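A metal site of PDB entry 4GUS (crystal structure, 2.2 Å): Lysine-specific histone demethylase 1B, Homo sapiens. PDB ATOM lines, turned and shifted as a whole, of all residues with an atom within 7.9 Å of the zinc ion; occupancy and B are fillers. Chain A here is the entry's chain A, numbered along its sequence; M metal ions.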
ATOM      1  N   LYS A   6       6.910  -4.940 -10.091  1.00  0.00           N
ATOM      2  CA  LYS A   6       5.677  -5.653  -9.757  1.00  0.00           C
ATOM      3  C   LYS A   6       5.324  -5.499  -8.269  1.00  0.00           C
ATOM      4  O   LYS A   6       6.189  -5.611  -7.396  1.00  0.00           O
ATOM      5  CB  LYS A   6       5.806  -7.129 -10.134  1.00  0.00           C
ATOM      6  CG  LYS A   6       4.474  -7.885 -10.161  1.00  0.00           C
ATOM      7  CD  LYS A   6       4.650  -9.283 -10.771  1.00  0.00           C
ATOM      8  CE  LYS A   6       5.086  -9.208 -12.235  1.00  0.00           C
ATOM      9  NZ  LYS A   6       5.429 -10.541 -12.812  1.00  0.00           N
ATOM     10  N   CYS A   7       4.042  -5.251  -7.998  1.00  0.00           N
ATOM     11  CA  CYS A   7       3.561  -5.114  -6.622  1.00  0.00           C
ATOM     12  C   CYS A   7       3.669  -6.442  -5.884  1.00  0.00           C
ATOM     13  O   CYS A   7       3.444  -7.500  -6.472  1.00  0.00           O
ATOM     14  CB  CYS A   7       2.121  -4.618  -6.600  1.00  0.00           C
ATOM     15  SG  CYS A   7       1.371  -4.524  -4.942  1.00  0.00           S
ATOM     16  N   GLU A   8       4.014  -6.368  -4.600  1.00  0.00           N
ATOM     17  CA  GLU A   8       4.083  -7.545  -3.709  1.00  0.00           C
ATOM     18  C   GLU A   8       2.757  -8.305  -3.643  1.00  0.00           C
ATOM     19  O   GLU A   8       2.740  -9.491  -3.307  1.00  0.00           O
ATOM     20  CB  GLU A   8       4.465  -7.108  -2.287  1.00  0.00           C
ATOM     21  CG  GLU A   8       3.344  -6.345  -1.558  1.00  0.00           C
ATOM     22  CD  GLU A   8       3.776  -5.680  -0.253  1.00  0.00           C
ATOM     23  OE1 GLU A   8       3.220  -4.608   0.078  1.00  0.00           O
ATOM     24  OE2 GLU A   8       4.668  -6.225   0.446  1.00  0.00           O
ATOM     25  N   LYS A   9       1.658  -7.624  -3.980  1.00  0.00           N
ATOM     26  CA  LYS A   9       0.313  -8.088  -3.670  1.00  0.00           C
ATOM     27  C   LYS A   9      -0.395  -8.771  -4.841  1.00  0.00           C
ATOM     28  O   LYS A   9      -0.681  -8.149  -5.872  1.00  0.00           O
ATOM     29  CB  LYS A   9      -0.526  -6.902  -3.158  1.00  0.00           C
ATOM     30  CG  LYS A   9      -2.030  -7.127  -3.091  1.00  0.00           C
ATOM     31  CD  LYS A   9      -2.452  -7.812  -1.811  1.00  0.00           C
ATOM     32  CE  LYS A   9      -3.963  -7.832  -1.681  1.00  0.00           C
ATOM     33  NZ  LYS A   9      -4.431  -8.810  -0.659  1.00  0.00           N
ATOM     34  N   ALA A  10      -0.681 -10.058  -4.661  1.00  0.00           N
ATOM     35  CA  ALA A  10      -1.376 -10.851  -5.673  1.00  0.00           C
ATOM     36  C   ALA A  10      -2.766 -10.311  -5.962  1.00  0.00           C
ATOM     37  O   ALA A  10      -3.628 -10.246  -5.071  1.00  0.00           O
ATOM     38  CB  ALA A  10      -1.440 -12.306  -5.266  1.00  0.00           C
ATOM     39  N   GLY A  11      -2.991  -9.924  -7.207  1.00  0.00           N
ATOM     40  CA  GLY A  11      -4.278  -9.427  -7.656  1.00  0.00           C
ATOM     41  C   GLY A  11      -4.310  -7.917  -7.848  1.00  0.00           C
ATOM     42  O   GLY A  11      -5.296  -7.372  -8.355  1.00  0.00           O
ATOM     43  N   CYS A  12      -3.228  -7.251  -7.437  1.00  0.00           N
ATOM     44  CA  CYS A  12      -3.179  -5.803  -7.538  1.00  0.00           C
ATOM     45  C   CYS A  12      -3.275  -5.413  -9.005  1.00  0.00           C
ATOM     46  O   CYS A  12      -2.678  -6.072  -9.867  1.00  0.00           O
ATOM     47  CB  CYS A  12      -1.905  -5.241  -6.890  1.00  0.00           C
ATOM     48  SG  CYS A  12      -1.819  -3.434  -6.937  1.00  0.00           S
ATOM     49  N   THR A  13      -4.033  -4.367  -9.289  1.00  0.00           N
ATOM     50  CA  THR A  13      -4.315  -3.971 -10.660  1.00  0.00           C
ATOM     51  C   THR A  13      -3.323  -2.936 -11.183  1.00  0.00           C
ATOM     52  O   THR A  13      -3.378  -2.527 -12.339  1.00  0.00           O
ATOM     53  CB  THR A  13      -5.742  -3.420 -10.786  1.00  0.00           C
ATOM     54  OG1 THR A  13      -5.921  -2.400  -9.804  1.00  0.00           O
ATOM     55  CG2 THR A  13      -6.742  -4.512 -10.524  1.00  0.00           C
ATOM     56  N   ALA A  14      -2.424  -2.492 -10.313  1.00  0.00           N
ATOM     57  CA  ALA A  14      -1.415  -1.536 -10.705  1.00  0.00           C
ATOM     58  C   ALA A  14      -0.368  -2.212 -11.590  1.00  0.00           C
ATOM     59  O   ALA A  14       0.370  -3.082 -11.136  1.00  0.00           O
ATOM     60  CB  ALA A  14      -0.751  -0.951  -9.472  1.00  0.00           C
ATOM     61  N   THR A  15      -0.310  -1.806 -12.862  1.00  0.00           N
ATOM     62  CA  THR A  15       0.712  -2.338 -13.780  1.00  0.00           C
ATOM     63  C   THR A  15       1.965  -1.475 -13.738  1.00  0.00           C
ATOM     64  O   THR A  15       3.050  -1.937 -14.068  1.00  0.00           O
ATOM     65  CB  THR A  15       0.226  -2.366 -15.238  1.00  0.00           C
ATOM     66  OG1 THR A  15      -0.175  -1.045 -15.621  1.00  0.00           O
ATOM     67  CG2 THR A  15      -0.950  -3.342 -15.407  1.00  0.00           C
ATOM     68  N   PRO A  17       3.542   0.665 -10.828  1.00  0.00           N
ATOM     69  CA  PRO A  17       3.625   1.221  -9.471  1.00  0.00           C
ATOM     70  C   PRO A  17       4.499   2.472  -9.416  1.00  0.00           C
ATOM     71  O   PRO A  17       5.582   2.500  -9.986  1.00  0.00           O
ATOM     72  CB  PRO A  17       4.281   0.088  -8.664  1.00  0.00           C
ATOM     73  CG  PRO A  17       4.132  -1.155  -9.497  1.00  0.00           C
ATOM     74  CD  PRO A  17       4.081  -0.698 -10.920  1.00  0.00           C
ATOM     75  N   TRP A  36       8.082  -3.436  -3.807  1.00  0.00           N
ATOM     76  CA  TRP A  36       7.052  -2.411  -3.810  1.00  0.00           C
ATOM     77  C   TRP A  36       6.068  -2.729  -2.703  1.00  0.00           C
ATOM     78  O   TRP A  36       5.485  -3.818  -2.661  1.00  0.00           O
ATOM     79  CB  TRP A  36       6.340  -2.384  -5.149  1.00  0.00           C
ATOM     80  CG  TRP A  36       7.053  -1.598  -6.168  1.00  0.00           C
ATOM     81  CD1 TRP A  36       7.705  -2.070  -7.262  1.00  0.00           C
ATOM     82  CD2 TRP A  36       7.196  -0.174  -6.189  1.00  0.00           C
ATOM     83  NE1 TRP A  36       8.250  -1.037  -7.978  1.00  0.00           N
ATOM     84  CE2 TRP A  36       7.954   0.147  -7.347  1.00  0.00           C
ATOM     85  CE3 TRP A  36       6.765   0.872  -5.365  1.00  0.00           C
ATOM     86  CZ2 TRP A  36       8.285   1.465  -7.692  1.00  0.00           C
ATOM     87  CZ3 TRP A  36       7.094   2.181  -5.706  1.00  0.00           C
ATOM     88  CH2 TRP A  36       7.844   2.461  -6.862  1.00  0.00           C
ATOM     89  N   TYR A  37       5.868  -1.783  -1.796  1.00  0.00           N
ATOM     90  CA  TYR A  37       4.938  -2.003  -0.699  1.00  0.00           C
ATOM     91  C   TYR A  37       3.547  -1.513  -1.076  1.00  0.00           C
ATOM     92  O   TYR A  37       3.389  -0.393  -1.551  1.00  0.00           O
ATOM     93  CB  TYR A  37       5.441  -1.326   0.560  1.00  0.00           C
ATOM     94  CG  TYR A  37       6.672  -1.990   1.086  1.00  0.00           C
ATOM     95  CD1 TYR A  37       6.585  -3.096   1.932  1.00  0.00           C
ATOM     96  CD2 TYR A  37       7.935  -1.554   0.707  1.00  0.00           C
ATOM     97  CE1 TYR A  37       7.712  -3.722   2.405  1.00  0.00           C
ATOM     98  CE2 TYR A  37       9.067  -2.185   1.173  1.00  0.00           C
ATOM     99  CZ  TYR A  37       8.949  -3.263   2.020  1.00  0.00           C
ATOM    100  OH  TYR A  37      10.091  -3.883   2.488  1.00  0.00           O
ATOM    101  N   HIS A  38       2.564  -2.379  -0.871  1.00  0.00           N
ATOM    102  CA  HIS A  38       1.186  -2.105  -1.284  1.00  0.00           C
ATOM    103  C   HIS A  38       0.318  -1.530  -0.161  1.00  0.00           C
ATOM    104  O   HIS A  38       0.093  -2.181   0.867  1.00  0.00           O
ATOM    105  CB  HIS A  38       0.558  -3.413  -1.785  1.00  0.00           C
ATOM    106  CG  HIS A  38      -0.890  -3.296  -2.154  1.00  0.00           C
ATOM    107  ND1 HIS A  38      -1.313  -3.096  -3.446  1.00  0.00           N
ATOM    108  CD2 HIS A  38      -2.014  -3.381  -1.400  1.00  0.00           C
ATOM    109  CE1 HIS A  38      -2.637  -3.061  -3.476  1.00  0.00           C
ATOM    110  NE2 HIS A  38      -3.086  -3.232  -2.240  1.00  0.00           N
ATOM    111  N   LEU A  39      -0.168  -0.303  -0.360  1.00  0.00           N
ATOM    112  CA  LEU A  39      -1.158   0.291   0.534  1.00  0.00           C
ATOM    113  C   LEU A  39      -2.543   0.064  -0.043  1.00  0.00           C
ATOM    114  O   LEU A  39      -3.424  -0.456   0.637  1.00  0.00           O
ATOM    115  CB  LEU A  39      -0.891   1.781   0.737  1.00  0.00           C
ATOM    116  CG  LEU A  39      -0.463   2.161   2.145  1.00  0.00           C
ATOM    117  CD1 LEU A  39       0.501   1.121   2.674  1.00  0.00           C
ATOM    118  CD2 LEU A  39       0.170   3.554   2.186  1.00  0.00           C
ATOM    119  N   SER A  40      -2.726   0.480  -1.282  1.00  0.00           N
ATOM    120  CA  SER A  40      -3.927   0.193  -2.055  1.00  0.00           C
ATOM    121  C   SER A  40      -3.513  -0.073  -3.499  1.00  0.00           C
ATOM    122  O   SER A  40      -2.320  -0.096  -3.817  1.00  0.00           O
ATOM    123  CB  SER A  40      -4.888   1.370  -2.015  1.00  0.00           C
ATOM    124  OG  SER A  40      -4.416   2.439  -2.828  1.00  0.00           O
ATOM    125  N   CYS A  41      -4.501  -0.262  -4.375  1.00  0.00           N
ATOM    126  CA  CYS A  41      -4.229  -0.493  -5.789  1.00  0.00           C
ATOM    127  C   CYS A  41      -3.610   0.708  -6.524  1.00  0.00           C
ATOM    128  O   CYS A  41      -2.938   0.531  -7.541  1.00  0.00           O
ATOM    129  CB  CYS A  41      -5.511  -0.959  -6.498  1.00  0.00           C
ATOM    130  SG  CYS A  41      -5.876  -2.679  -6.152  1.00  0.00           S
ATOM    131  N   GLY A  42      -3.862   1.906  -6.021  1.00  0.00           N
ATOM    132  CA  GLY A  42      -3.310   3.117  -6.603  1.00  0.00           C
ATOM    133  C   GLY A  42      -2.124   3.699  -5.841  1.00  0.00           C
ATOM    134  O   GLY A  42      -1.569   4.735  -6.221  1.00  0.00           O
ATOM    135  N   GLU A  43      -1.732   3.039  -4.757  1.00  0.00           N
ATOM    136  CA  GLU A  43      -0.768   3.603  -3.815  1.00  0.00           C
ATOM    137  C   GLU A  43       0.256   2.593  -3.323  1.00  0.00           C
ATOM    138  O   GLU A  43      -0.080   1.637  -2.632  1.00  0.00           O
ATOM    139  CB  GLU A  43      -1.499   4.231  -2.619  1.00  0.00           C
ATOM    140  CG  GLU A  43      -2.299   5.471  -3.007  1.00  0.00           C
ATOM    141  CD  GLU A  43      -3.492   5.717  -2.101  1.00  0.00           C
ATOM    142  OE1 GLU A  43      -3.891   6.884  -1.949  1.00  0.00           O
ATOM    143  OE2 GLU A  43      -4.038   4.735  -1.545  1.00  0.00           O
ATOM    144  N   HIS A  44       1.526   2.837  -3.686  1.00  0.00           N
ATOM    145  CA  HIS A  44       2.640   1.984  -3.280  1.00  0.00           C
ATOM    146  C   HIS A  44       3.801   2.865  -2.854  1.00  0.00           C
ATOM    147  O   HIS A  44       3.848   4.050  -3.179  1.00  0.00           O
ATOM    148  CB  HIS A  44       3.074   1.078  -4.440  1.00  0.00           C
ATOM    149  CG  HIS A  44       1.946   0.333  -5.074  1.00  0.00           C
ATOM    150  ND1 HIS A  44       1.016   0.944  -5.887  1.00  0.00           N
ATOM    151  CD2 HIS A  44       1.557  -0.972  -4.973  1.00  0.00           C
ATOM    152  CE1 HIS A  44       0.109   0.055  -6.264  1.00  0.00           C
ATOM    153  NE2 HIS A  44       0.415  -1.105  -5.725  1.00  0.00           N
ATOM    154  N   MET A 158      -8.948  -4.756  -1.456  1.00  0.00           N
ATOM    155  CA  MET A 158      -7.483  -4.756  -1.571  1.00  0.00           C
ATOM    156  C   MET A 158      -6.780  -3.579  -0.888  1.00  0.00           C
ATOM    157  O   MET A 158      -5.568  -3.371  -1.049  1.00  0.00           O
ATOM    158  CB  MET A 158      -7.053  -4.899  -3.029  1.00  0.00           C
ATOM    159  CG  MET A 158      -7.086  -6.362  -3.464  1.00  0.00           C
ATOM    160  SD  MET A 158      -6.356  -6.611  -5.079  1.00  0.00           S
ATOM    161  CE  MET A 158      -7.519  -5.714  -6.082  1.00  0.00           C
ATOM    162  N   ILE A 160      -5.238  -2.395   2.298  1.00  0.00           N
ATOM    163  CA  ILE A 160      -4.655  -3.191   3.394  1.00  0.00           C
ATOM    164  C   ILE A 160      -5.184  -2.793   4.793  1.00  0.00           C
ATOM    165  O   ILE A 160      -5.563  -3.637   5.600  1.00  0.00           O
ATOM    166  CB  ILE A 160      -3.104  -3.116   3.382  1.00  0.00           C
ATOM    167  CG1 ILE A 160      -2.570  -3.584   2.026  1.00  0.00           C
ATOM    168  CG2 ILE A 160      -2.510  -3.949   4.523  1.00  0.00           C
ATOM    169  CD1 ILE A 160      -3.206  -4.893   1.519  1.00  0.00           C
HETATM  170 ZN    ZN M   1      -0.265  -3.067  -5.293  1.00  0.00          ZN
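A ring nitrogen (NE2) of His 44 sits close to the backbone carbonyl oxygen (O) of Ser 40 (3.5 Å). The side-chain carboxylate (OE2) of Glu 43 is in hydrogen-bond range of the side-chain hydroxyl (OG) of Ser 40 (2.7 Å). The backbone carbonyl oxygen of Ser 40 sits close to a ring nitrogen (ND1) of His 38 (3.2 Å). N of His 38 lies within hydrogen-bond range of OE1 of Glu 8. N of Ala 14 sits close to SG of Cys 12, at 3.6 Å. OG of Ser 40 sits close to N of Gly 42, 3.3 Å away. N of Lys 9 sits close to SG of Cys 7, at 3.3 Å. A ring nitrogen (NE2) of His 38 is in hydrogen-bond range of the backbone carbonyl oxygen of Met 158, 2.8 Å away.
Merely in contact with the zinc ion: Ser 40 (3.9 Å). Five residues have an atom within 4 Å of the zinc ion: Cys 7, Cys 12, His 38, Ser 40 and His 44. The nearest printed residue that does not touch the zinc ion is Lys 9 (4.4 Å).
The zinc ion is bound by a ring nitrogen (NE2) of His 44, at 2.1 Å. The zinc ion is bound by a ring nitrogen (ND1) of His 38 (2.1 Å). The zinc ion is bound by the side-chain sulfur (SG) of Cys 7. SG of Cys 12 binds the zinc ion, 2.3 Å away. The zinc ion has four donor atoms within binding distance.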
